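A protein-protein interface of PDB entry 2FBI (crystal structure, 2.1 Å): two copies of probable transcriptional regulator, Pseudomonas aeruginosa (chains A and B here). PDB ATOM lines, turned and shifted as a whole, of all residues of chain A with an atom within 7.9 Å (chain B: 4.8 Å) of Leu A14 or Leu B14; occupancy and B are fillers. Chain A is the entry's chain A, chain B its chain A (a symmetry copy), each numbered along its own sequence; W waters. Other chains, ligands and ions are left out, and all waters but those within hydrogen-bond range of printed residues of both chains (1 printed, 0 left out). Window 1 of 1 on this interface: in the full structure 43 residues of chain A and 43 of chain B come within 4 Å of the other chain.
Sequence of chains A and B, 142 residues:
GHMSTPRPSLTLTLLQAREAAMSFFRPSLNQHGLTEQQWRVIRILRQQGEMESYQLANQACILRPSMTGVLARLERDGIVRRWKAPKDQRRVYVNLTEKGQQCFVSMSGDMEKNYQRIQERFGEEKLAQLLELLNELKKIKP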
ATOM      1  N   SER A   9     -17.113  16.460 -15.383  1.00  0.00           N
ATOM      2  CA  SER A   9     -16.867  15.413 -14.422  1.00  0.00           C
ATOM      3  C   SER A   9     -15.821  14.516 -15.005  1.00  0.00           C
ATOM      4  O   SER A   9     -16.071  13.820 -16.009  1.00  0.00           O
ATOM      5  CB  SER A   9     -18.127  14.648 -14.129  1.00  0.00           C
ATOM      6  OG  SER A   9     -17.847  13.545 -13.295  1.00  0.00           O
ATOM      7  N   LEU A  10     -14.606  14.590 -14.428  1.00  0.00           N
ATOM      8  CA  LEU A  10     -13.558  13.620 -14.747  1.00  0.00           C
ATOM      9  C   LEU A  10     -14.033  12.167 -14.614  1.00  0.00           C
ATOM     10  O   LEU A  10     -13.795  11.325 -15.479  1.00  0.00           O
ATOM     11  CB  LEU A  10     -12.390  13.771 -13.783  1.00  0.00           C
ATOM     12  CG  LEU A  10     -11.213  12.812 -14.050  1.00  0.00           C
ATOM     13  CD1 LEU A  10     -10.662  13.043 -15.461  1.00  0.00           C
ATOM     14  CD2 LEU A  10     -10.084  12.984 -12.991  1.00  0.00           C
ATOM     15  N   THR A  11     -14.678  11.864 -13.495  1.00  0.00           N
ATOM     16  CA  THR A  11     -15.003  10.496 -13.215  1.00  0.00           C
ATOM     17  C   THR A  11     -16.195   9.982 -14.082  1.00  0.00           C
ATOM     18  O   THR A  11     -16.172   8.823 -14.542  1.00  0.00           O
ATOM     19  CB  THR A  11     -15.380  10.338 -11.742  1.00  0.00           C
ATOM     20  OG1 THR A  11     -16.403  11.271 -11.459  1.00  0.00           O
ATOM     21  CG2 THR A  11     -14.169  10.625 -10.776  1.00  0.00           C
ATOM     22  N   LEU A  12     -17.257  10.769 -14.228  1.00  0.00           N
ATOM     23  CA  LEU A  12     -18.317  10.378 -15.191  1.00  0.00           C
ATOM     24  C   LEU A  12     -17.729  10.245 -16.600  1.00  0.00           C
ATOM     25  O   LEU A  12     -17.984   9.245 -17.281  1.00  0.00           O
ATOM     26  CB  LEU A  12     -19.510  11.345 -15.133  1.00  0.00           C
ATOM     27  CG  LEU A  12     -20.794  11.158 -15.973  1.00  0.00           C
ATOM     28  CD1 LEU A  12     -21.275   9.723 -16.014  1.00  0.00           C
ATOM     29  CD2 LEU A  12     -21.882  12.091 -15.324  1.00  0.00           C
ATOM     30  N   THR A  13     -16.846  11.169 -16.993  1.00  0.00           N
ATOM     31  CA  THR A  13     -16.182  11.120 -18.333  1.00  0.00           C
ATOM     32  C   THR A  13     -15.297   9.872 -18.545  1.00  0.00           C
ATOM     33  O   THR A  13     -15.302   9.258 -19.623  1.00  0.00           O
ATOM     34  CB  THR A  13     -15.410  12.428 -18.620  1.00  0.00           C
ATOM     35  OG1 THR A  13     -16.356  13.485 -18.643  1.00  0.00           O
ATOM     36  CG2 THR A  13     -14.704  12.429 -19.953  1.00  0.00           C
ATOM     37  N   LEU A  14     -14.549   9.470 -17.515  1.00  0.00           N
ATOM     38  CA  LEU A  14     -13.849   8.161 -17.533  1.00  0.00           C
ATOM     39  C   LEU A  14     -14.771   6.970 -17.846  1.00  0.00           C
ATOM     40  O   LEU A  14     -14.413   6.076 -18.585  1.00  0.00           O
ATOM     41  CB  LEU A  14     -13.179   7.901 -16.162  1.00  0.00           C
ATOM     42  CG  LEU A  14     -11.865   8.701 -16.013  1.00  0.00           C
ATOM     43  CD1 LEU A  14     -11.504   8.988 -14.539  1.00  0.00           C
ATOM     44  CD2 LEU A  14     -10.760   7.983 -16.710  1.00  0.00           C
ATOM     45  N   LEU A  15     -15.931   6.969 -17.225  1.00  0.00           N
ATOM     46  CA  LEU A  15     -16.893   5.916 -17.340  1.00  0.00           C
ATOM     47  C   LEU A  15     -17.632   5.911 -18.743  1.00  0.00           C
ATOM     48  O   LEU A  15     -17.823   4.856 -19.355  1.00  0.00           O
ATOM     49  CB  LEU A  15     -17.847   6.128 -16.182  1.00  0.00           C
ATOM     50  CG  LEU A  15     -18.434   5.016 -15.334  1.00  0.00           C
ATOM     51  CD1 LEU A  15     -17.503   3.799 -15.015  1.00  0.00           C
ATOM     52  CD2 LEU A  15     -19.054   5.593 -14.066  1.00  0.00           C
ATOM     53  N   GLN A  16     -17.986   7.078 -19.244  1.00  0.00           N
ATOM     54  CA  GLN A  16     -18.504   7.227 -20.645  1.00  0.00           C
ATOM     55  C   GLN A  16     -17.458   6.848 -21.697  1.00  0.00           C
ATOM     56  O   GLN A  16     -17.755   6.085 -22.609  1.00  0.00           O
ATOM     57  CB  GLN A  16     -19.016   8.651 -20.876  1.00  0.00           C
ATOM     58  CG  GLN A  16     -20.145   9.080 -19.930  1.00  0.00           C
ATOM     59  CD  GLN A  16     -20.408  10.586 -19.992  1.00  0.00           C
ATOM     60  OE1 GLN A  16     -19.503  11.365 -20.186  1.00  0.00           O
ATOM     61  NE2 GLN A  16     -21.639  10.990 -19.758  1.00  0.00           N
ATOM     62  N   ALA A  17     -16.205   7.318 -21.542  1.00  0.00           N
ATOM     63  CA  ALA A  17     -15.136   6.802 -22.390  1.00  0.00           C
ATOM     64  C   ALA A  17     -15.003   5.280 -22.352  1.00  0.00           C
ATOM     65  O   ALA A  17     -14.794   4.661 -23.403  1.00  0.00           O
ATOM     66  CB  ALA A  17     -13.798   7.482 -22.112  1.00  0.00           C
ATOM     67  N   ARG A  18     -15.170   4.672 -21.177  1.00  0.00           N
ATOM     68  CA  ARG A  18     -15.107   3.214 -21.068  1.00  0.00           C
ATOM     69  C   ARG A  18     -16.305   2.530 -21.780  1.00  0.00           C
ATOM     70  O   ARG A  18     -16.147   1.435 -22.329  1.00  0.00           O
ATOM     71  CB  ARG A  18     -15.034   2.749 -19.580  1.00  0.00           C
ATOM     72  CG  ARG A  18     -15.021   1.208 -19.395  1.00  0.00           C
ATOM     73  CD  ARG A  18     -15.411   0.701 -17.926  1.00  0.00           C
ATOM     74  NE  ARG A  18     -15.500  -0.765 -17.873  1.00  0.00           N
ATOM     75  CZ  ARG A  18     -16.643  -1.445 -17.943  1.00  0.00           C
ATOM     76  NH1 ARG A  18     -17.807  -0.814 -18.073  1.00  0.00           N
ATOM     77  NH2 ARG A  18     -16.652  -2.759 -17.884  1.00  0.00           N
ATOM     78  N   GLU A  19     -17.482   3.148 -21.744  1.00  0.00           N
ATOM     79  CA  GLU A  19     -18.681   2.589 -22.455  1.00  0.00           C
ATOM     80  C   GLU A  19     -18.421   2.627 -23.936  1.00  0.00           C
ATOM     81  O   GLU A  19     -18.545   1.631 -24.601  1.00  0.00           O
ATOM     82  CB  GLU A  19     -19.962   3.365 -22.125  1.00  0.00           C
ATOM     83  CG  GLU A  19     -20.487   3.126 -20.746  1.00  0.00           C
ATOM     84  CD  GLU A  19     -20.880   1.654 -20.522  1.00  0.00           C
ATOM     85  OE1 GLU A  19     -21.597   1.067 -21.385  1.00  0.00           O
ATOM     86  OE2 GLU A  19     -20.443   1.075 -19.498  1.00  0.00           O
ATOM     87  N   ALA A  20     -17.977   3.769 -24.437  1.00  0.00           N
ATOM     88  CA  ALA A  20     -17.446   3.836 -25.817  1.00  0.00           C
ATOM     89  C   ALA A  20     -16.507   2.665 -26.213  1.00  0.00           C
ATOM     90  O   ALA A  20     -16.819   1.910 -27.125  1.00  0.00           O
ATOM     91  CB  ALA A  20     -16.821   5.168 -26.065  1.00  0.00           C
ATOM     92  N   ALA A  21     -15.408   2.448 -25.487  1.00  0.00           N
ATOM     93  CA  ALA A  21     -14.521   1.328 -25.788  1.00  0.00           C
ATOM     94  C   ALA A  21     -15.155  -0.026 -25.647  1.00  0.00           C
ATOM     95  O   ALA A  21     -14.842  -0.933 -26.450  1.00  0.00           O
ATOM     96  CB  ALA A  21     -13.225   1.395 -24.897  1.00  0.00           C
ATOM     97  N   MET A  22     -16.026  -0.190 -24.634  1.00  0.00           N
ATOM     98  CA  MET A  22     -16.709  -1.465 -24.394  1.00  0.00           C
ATOM     99  C   MET A  22     -17.639  -1.918 -25.520  1.00  0.00           C
ATOM    100  O   MET A  22     -17.883  -3.116 -25.665  1.00  0.00           O
ATOM    101  CB  MET A  22     -17.464  -1.552 -23.043  1.00  0.00           C
ATOM    102  CG  MET A  22     -16.560  -1.719 -21.800  1.00  0.00           C
ATOM    103  SD  MET A  22     -15.560  -3.225 -21.707  1.00  0.00           S
ATOM    104  CE  MET A  22     -16.790  -4.499 -21.769  1.00  0.00           C
ATOM    105  N   CYS A  61     -11.821  -4.243  -9.879  1.00  0.00           N
ATOM    106  CA  CYS A  61     -12.855  -3.248  -9.766  1.00  0.00           C
ATOM    107  C   CYS A  61     -14.234  -3.950  -9.804  1.00  0.00           C
ATOM    108  O   CYS A  61     -15.026  -3.786 -10.756  1.00  0.00           O
ATOM    109  CB  CYS A  61     -12.690  -2.204 -10.881  1.00  0.00           C
ATOM    110  SG  CYS A  61     -11.263  -1.096 -10.625  1.00  0.00           S
ATOM    111  N   TYR A 115      -8.992  -4.311 -30.350  1.00  0.00           N
ATOM    112  CA  TYR A 115      -8.031  -3.233 -30.064  1.00  0.00           C
ATOM    113  C   TYR A 115      -7.452  -2.589 -31.332  1.00  0.00           C
ATOM    114  O   TYR A 115      -7.235  -1.395 -31.360  1.00  0.00           O
ATOM    115  CB  TYR A 115      -6.872  -3.708 -29.141  1.00  0.00           C
ATOM    116  CG  TYR A 115      -7.216  -3.544 -27.693  1.00  0.00           C
ATOM    117  CD1 TYR A 115      -7.431  -4.656 -26.890  1.00  0.00           C
ATOM    118  CD2 TYR A 115      -7.416  -2.249 -27.140  1.00  0.00           C
ATOM    119  CE1 TYR A 115      -7.775  -4.503 -25.529  1.00  0.00           C
ATOM    120  CE2 TYR A 115      -7.773  -2.095 -25.809  1.00  0.00           C
ATOM    121  CZ  TYR A 115      -7.947  -3.227 -25.005  1.00  0.00           C
ATOM    122  OH  TYR A 115      -8.322  -3.084 -23.692  1.00  0.00           O
ATOM    123  N   LEU A 130      -3.126   8.246 -23.950  1.00  0.00           N
ATOM    124  CA  LEU A 130      -4.215   8.094 -23.030  1.00  0.00           C
ATOM    125  C   LEU A 130      -3.822   7.118 -21.889  1.00  0.00           C
ATOM    126  O   LEU A 130      -4.039   7.423 -20.715  1.00  0.00           O
ATOM    127  CB  LEU A 130      -5.501   7.602 -23.750  1.00  0.00           C
ATOM    128  CG  LEU A 130      -6.631   7.278 -22.770  1.00  0.00           C
ATOM    129  CD1 LEU A 130      -6.994   8.565 -21.977  1.00  0.00           C
ATOM    130  CD2 LEU A 130      -7.843   6.654 -23.475  1.00  0.00           C
ATOM    131  N   LEU A 131      -3.335   5.945 -22.283  1.00  0.00           N
ATOM    132  CA  LEU A 131      -2.874   4.895 -21.389  1.00  0.00           C
ATOM    133  C   LEU A 131      -1.752   5.352 -20.464  1.00  0.00           C
ATOM    134  O   LEU A 131      -1.776   5.034 -19.271  1.00  0.00           O
ATOM    135  CB  LEU A 131      -2.424   3.662 -22.167  1.00  0.00           C
ATOM    136  CG  LEU A 131      -3.571   2.898 -22.796  1.00  0.00           C
ATOM    137  CD1 LEU A 131      -3.063   2.058 -23.929  1.00  0.00           C
ATOM    138  CD2 LEU A 131      -4.305   2.039 -21.729  1.00  0.00           C
ATOM    139  N   LEU A 134      -3.502   7.689 -18.042  1.00  0.00           N
ATOM    140  CA  LEU A 134      -4.338   6.965 -17.113  1.00  0.00           C
ATOM    141  C   LEU A 134      -3.473   6.206 -16.086  1.00  0.00           C
ATOM    142  O   LEU A 134      -3.826   6.107 -14.934  1.00  0.00           O
ATOM    143  CB  LEU A 134      -5.225   5.972 -17.861  1.00  0.00           C
ATOM    144  CG  LEU A 134      -6.411   6.487 -18.708  1.00  0.00           C
ATOM    145  CD1 LEU A 134      -6.902   5.342 -19.529  1.00  0.00           C
ATOM    146  CD2 LEU A 134      -7.506   7.067 -17.817  1.00  0.00           C
ATOM    147  N   ASN A 135      -2.365   5.648 -16.545  1.00  0.00           N
ATOM    148  CA  ASN A 135      -1.408   4.999 -15.652  1.00  0.00           C
ATOM    149  C   ASN A 135      -0.872   5.984 -14.597  1.00  0.00           C
ATOM    150  O   ASN A 135      -0.776   5.643 -13.425  1.00  0.00           O
ATOM    151  CB  ASN A 135      -0.341   4.252 -16.461  1.00  0.00           C
ATOM    152  CG  ASN A 135      -0.838   2.867 -16.927  1.00  0.00           C
ATOM    153  OD1 ASN A 135      -1.672   2.220 -16.242  1.00  0.00           O
ATOM    154  ND2 ASN A 135      -0.315   2.392 -18.081  1.00  0.00           N
ATOM    155  N   LEU A 137      -2.615   8.820 -13.637  1.00  0.00           N
ATOM    156  CA  LEU A 137      -3.745   9.153 -12.761  1.00  0.00           C
ATOM    157  C   LEU A 137      -3.936   8.143 -11.624  1.00  0.00           C
ATOM    158  O   LEU A 137      -4.370   8.505 -10.550  1.00  0.00           O
ATOM    159  CB  LEU A 137      -5.072   9.313 -13.550  1.00  0.00           C
ATOM    160  CG  LEU A 137      -6.302   9.845 -12.797  1.00  0.00           C
ATOM    161  CD1 LEU A 137      -6.029  11.229 -12.180  1.00  0.00           C
ATOM    162  CD2 LEU A 137      -7.474   9.956 -13.756  1.00  0.00           C
ATOM    163  N   LYS A 138      -3.690   6.880 -11.896  1.00  0.00           N
ATOM    164  CA  LYS A 138      -3.828   5.860 -10.882  1.00  0.00           C
ATOM    165  C   LYS A 138      -2.833   6.102  -9.740  1.00  0.00           C
ATOM    166  O   LYS A 138      -3.120   5.783  -8.602  1.00  0.00           O
ATOM    167  CB  LYS A 138      -3.611   4.470 -11.461  1.00  0.00           C
ATOM    168  CG  LYS A 138      -4.482   4.150 -12.674  1.00  0.00           C
ATOM    169  CD  LYS A 138      -4.673   2.703 -12.832  1.00  0.00           C
ATOM    170  CE  LYS A 138      -3.535   1.871 -12.265  1.00  0.00           C
ATOM    171  NZ  LYS A 138      -3.482   0.544 -12.926  1.00  0.00           N
ATOM    172  N   LEU B  10      -7.187  -1.271 -21.708  1.00  0.00           N
ATOM    173  CA  LEU B  10      -7.724   0.091 -21.719  1.00  0.00           C
ATOM    174  C   LEU B  10      -8.918   0.267 -20.771  1.00  0.00           C
ATOM    175  O   LEU B  10      -9.001   1.227 -20.006  1.00  0.00           O
ATOM    176  CB  LEU B  10      -8.235   0.442 -23.110  1.00  0.00           C
ATOM    177  CG  LEU B  10      -8.798   1.871 -23.241  1.00  0.00           C
ATOM    178  CD1 LEU B  10      -7.711   2.893 -22.891  1.00  0.00           C
ATOM    179  CD2 LEU B  10      -9.355   2.137 -24.672  1.00  0.00           C
ATOM    180  N   THR B  11      -9.870  -0.653 -20.855  1.00  0.00           N
ATOM    181  CA  THR B  11     -11.093  -0.470 -20.130  1.00  0.00           C
ATOM    182  C   THR B  11     -10.922  -0.737 -18.602  1.00  0.00           C
ATOM    183  O   THR B  11     -11.509  -0.010 -17.776  1.00  0.00           O
ATOM    184  CB  THR B  11     -12.165  -1.422 -20.664  1.00  0.00           C
ATOM    185  OG1 THR B  11     -11.633  -2.730 -20.630  1.00  0.00           O
ATOM    186  CG2 THR B  11     -12.574  -1.095 -22.150  1.00  0.00           C
ATOM    187  N   LEU B  12     -10.224  -1.803 -18.219  1.00  0.00           N
ATOM    188  CA  LEU B  12      -9.897  -1.972 -16.783  1.00  0.00           C
ATOM    189  C   LEU B  12      -9.089  -0.772 -16.278  1.00  0.00           C
ATOM    190  O   LEU B  12      -9.411  -0.213 -15.223  1.00  0.00           O
ATOM    191  CB  LEU B  12      -9.192  -3.314 -16.523  1.00  0.00           C
ATOM    192  CG  LEU B  12      -8.789  -3.800 -15.112  1.00  0.00           C
ATOM    193  CD1 LEU B  12      -9.855  -3.550 -14.067  1.00  0.00           C
ATOM    194  CD2 LEU B  12      -8.492  -5.340 -15.249  1.00  0.00           C
ATOM    195  N   THR B  13      -8.133  -0.288 -17.077  1.00  0.00           N
ATOM    196  CA  THR B  13      -7.306   0.902 -16.703  1.00  0.00           C
ATOM    197  C   THR B  13      -8.123   2.201 -16.535  1.00  0.00           C
ATOM    198  O   THR B  13      -7.895   2.986 -15.602  1.00  0.00           O
ATOM    199  CB  THR B  13      -6.125   1.089 -17.683  1.00  0.00           C
ATOM    200  OG1 THR B  13      -5.301  -0.061 -17.582  1.00  0.00           O
ATOM    201  CG2 THR B  13      -5.264   2.287 -17.366  1.00  0.00           C
ATOM    202  N   LEU B  14      -9.099   2.430 -17.419  1.00  0.00           N
ATOM    203  CA  LEU B  14     -10.088   3.518 -17.212  1.00  0.00           C
ATOM    204  C   LEU B  14     -10.792   3.464 -15.846  1.00  0.00           C
ATOM    205  O   LEU B  14     -10.997   4.475 -15.205  1.00  0.00           O
ATOM    206  CB  LEU B  14     -11.174   3.459 -18.315  1.00  0.00           C
ATOM    207  CG  LEU B  14     -10.663   4.055 -19.646  1.00  0.00           C
ATOM    208  CD1 LEU B  14     -11.399   3.481 -20.876  1.00  0.00           C
ATOM    209  CD2 LEU B  14     -10.764   5.542 -19.599  1.00  0.00           C
ATOM    210  N   LEU B  15     -11.190   2.272 -15.456  1.00  0.00           N
ATOM    211  CA  LEU B  15     -11.916   2.034 -14.247  1.00  0.00           C
ATOM    212  C   LEU B  15     -11.011   2.166 -12.953  1.00  0.00           C
ATOM    213  O   LEU B  15     -11.420   2.761 -11.951  1.00  0.00           O
ATOM    214  CB  LEU B  15     -12.500   0.644 -14.408  1.00  0.00           C
ATOM    215  CG  LEU B  15     -13.896   0.240 -13.972  1.00  0.00           C
ATOM    216  CD1 LEU B  15     -15.033   1.299 -14.157  1.00  0.00           C
ATOM    217  CD2 LEU B  15     -14.272  -1.100 -14.592  1.00  0.00           C
ATOM    218  N   GLN B  16      -9.795   1.658 -13.009  1.00  0.00           N
ATOM    219  CA  GLN B  16      -8.774   1.894 -11.934  1.00  0.00           C
ATOM    220  C   GLN B  16      -8.387   3.370 -11.812  1.00  0.00           C
ATOM    221  O   GLN B  16      -8.379   3.912 -10.711  1.00  0.00           O
ATOM    222  CB  GLN B  16      -7.538   1.024 -12.173  1.00  0.00           C
ATOM    223  CG  GLN B  16      -7.818  -0.483 -12.204  1.00  0.00           C
ATOM    224  CD  GLN B  16      -6.628  -1.280 -12.744  1.00  0.00           C
ATOM    225  OE1 GLN B  16      -5.912  -0.818 -13.602  1.00  0.00           O
ATOM    226  NE2 GLN B  16      -6.467  -2.503 -12.285  1.00  0.00           N
ATOM    227  N   ALA B  17      -8.133   4.054 -12.945  1.00  0.00           N
ATOM    228  CA  ALA B  17      -7.981   5.504 -12.886  1.00  0.00           C
ATOM    229  C   ALA B  17      -9.168   6.220 -12.242  1.00  0.00           C
ATOM    230  O   ALA B  17      -8.961   7.157 -11.460  1.00  0.00           O
ATOM    231  CB  ALA B  17      -7.645   6.104 -14.250  1.00  0.00           C
ATOM    232  N   ARG B  18     -10.391   5.764 -12.515  1.00  0.00           N
ATOM    233  CA  ARG B  18     -11.574   6.364 -11.900  1.00  0.00           C
ATOM    234  C   ARG B  18     -11.632   6.087 -10.372  1.00  0.00           C
ATOM    235  O   ARG B  18     -12.113   6.935  -9.614  1.00  0.00           O
ATOM    236  CB  ARG B  18     -12.891   5.877 -12.581  1.00  0.00           C
ATOM    237  CG  ARG B  18     -14.186   6.437 -11.934  1.00  0.00           C
ATOM    238  CD  ARG B  18     -15.521   5.624 -12.284  1.00  0.00           C
ATOM    239  NE  ARG B  18     -16.674   6.139 -11.534  1.00  0.00           N
ATOM    240  CZ  ARG B  18     -17.144   5.585 -10.417  1.00  0.00           C
ATOM    241  NH1 ARG B  18     -16.575   4.499  -9.902  1.00  0.00           N
ATOM    242  NH2 ARG B  18     -18.184   6.096  -9.794  1.00  0.00           N
ATOM    243  N   LEU B 134     -10.150  11.860 -23.371  1.00  0.00           N
ATOM    244  CA  LEU B 134     -11.301  11.065 -23.013  1.00  0.00           C
ATOM    245  C   LEU B 134     -12.546  11.531 -23.793  1.00  0.00           C
ATOM    246  O   LEU B 134     -13.365  10.734 -24.185  1.00  0.00           O
ATOM    247  CB  LEU B 134     -11.572  11.171 -21.513  1.00  0.00           C
ATOM    248  CG  LEU B 134     -10.628  10.471 -20.510  1.00  0.00           C
ATOM    249  CD1 LEU B 134     -10.970  10.979 -19.150  1.00  0.00           C
ATOM    250  CD2 LEU B 134     -10.758   8.952 -20.607  1.00  0.00           C
ATOM    251  N   LEU B 137     -12.138   9.887 -27.064  1.00  0.00           N
ATOM    252  CA  LEU B 137     -12.445   8.453 -27.006  1.00  0.00           C
ATOM    253  C   LEU B 137     -13.950   8.165 -27.045  1.00  0.00           C
ATOM    254  O   LEU B 137     -14.367   7.152 -27.566  1.00  0.00           O
ATOM    255  CB  LEU B 137     -11.810   7.765 -25.770  1.00  0.00           C
ATOM    256  CG  LEU B 137     -11.887   6.233 -25.676  1.00  0.00           C
ATOM    257  CD1 LEU B 137     -11.231   5.559 -26.896  1.00  0.00           C
ATOM    258  CD2 LEU B 137     -11.178   5.766 -24.415  1.00  0.00           C
HETATM  259  O   HOH W   1      -2.161  -0.330 -18.434  1.00  0.00           O
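OG of Ser A9 sits at hydrogen-bond distance from OG1 of Thr A11, 3.3 Å away.
O of Ser A9 lies within hydrogen-bond range of OG1 of Thr A13.
OE2 of Glu A19 is in salt-bridge range of NH1 of Arg A18 (3.5 Å).
The backbone carbonyl oxygen (O) of Leu A131 sits at hydrogen-bond distance from the side-chain amide nitrogen (ND2) of Asn A135, 3.2 Å away.
Leu B14 touches Leu A14 (CD2 to CD2, 3.8 Å).
Leu A14 touches Arg B18.
CB of Ala A17 touches CD2 of Leu B137, at 3.9 Å.
Arg A18 touches Leu B15 (NE to CD2, 3.5 Å).
SD of Met A22 touches CG2 of Thr B11, 3.7 Å away.
CD2 of Leu A130 touches CD2 of Leu B137, at 3.6 Å.
Leu A131 touches Leu B10 (CD2 to CD1, 3.7 Å).
CB of Leu A134 touches CG2 of Thr B13 (3.7 Å).
OD1 of Asn A135 touches CG2 of Thr B13, 3.8 Å away.
Leu A137 touches Ala B17.
Water W1 bridges OG1 of Thr B13 and ND2 of Asn A135.
Of the printed residues of chain B, Leu A14 touches Leu B14, Arg B18 and Leu B134.
Leu B14 touches just these residues of chain A: Leu A14 (3.8 Å), Arg A18 (3.7 Å) and Leu A134 (3.9 Å).
Printed residues of chain B within 4 Å of Thr A13: Leu B134 (3.7 Å).
Of the printed residues of chain B, Leu A131 touches Leu B10 (3.7 Å).
Leu A12 touches none of the printed residues of chain B.
Glu A19 touches none of the printed residues of chain B.
The nearest residue of chain B that does not touch Leu A14 is Ala B17 (4.3 Å).
The nearest residue of chain A that does not touch Leu B14 is Ala A17 (4.3 Å).
The side-chain hydroxyl of Tyr A115 lies within hydrogen-bond range of the backbone NH of Leu B10.
The side-chain amino group (NZ) of Lys A138 is in hydrogen-bond range of the side-chain amide oxygen (OE1) of Gln B16 (2.9 Å).
Thr A13 touches Leu B134, and with the chains exchanged Leu A134 touches Thr B13.
Leu A14 touches Arg B18, and with the chains exchanged Arg A18 touches Leu B14.
Leu A14 touches Leu B134, and with the chains exchanged Leu A134 touches Leu B14.
Ala A17 touches Leu B137, and with the chains exchanged Leu A137 touches Ala B17.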
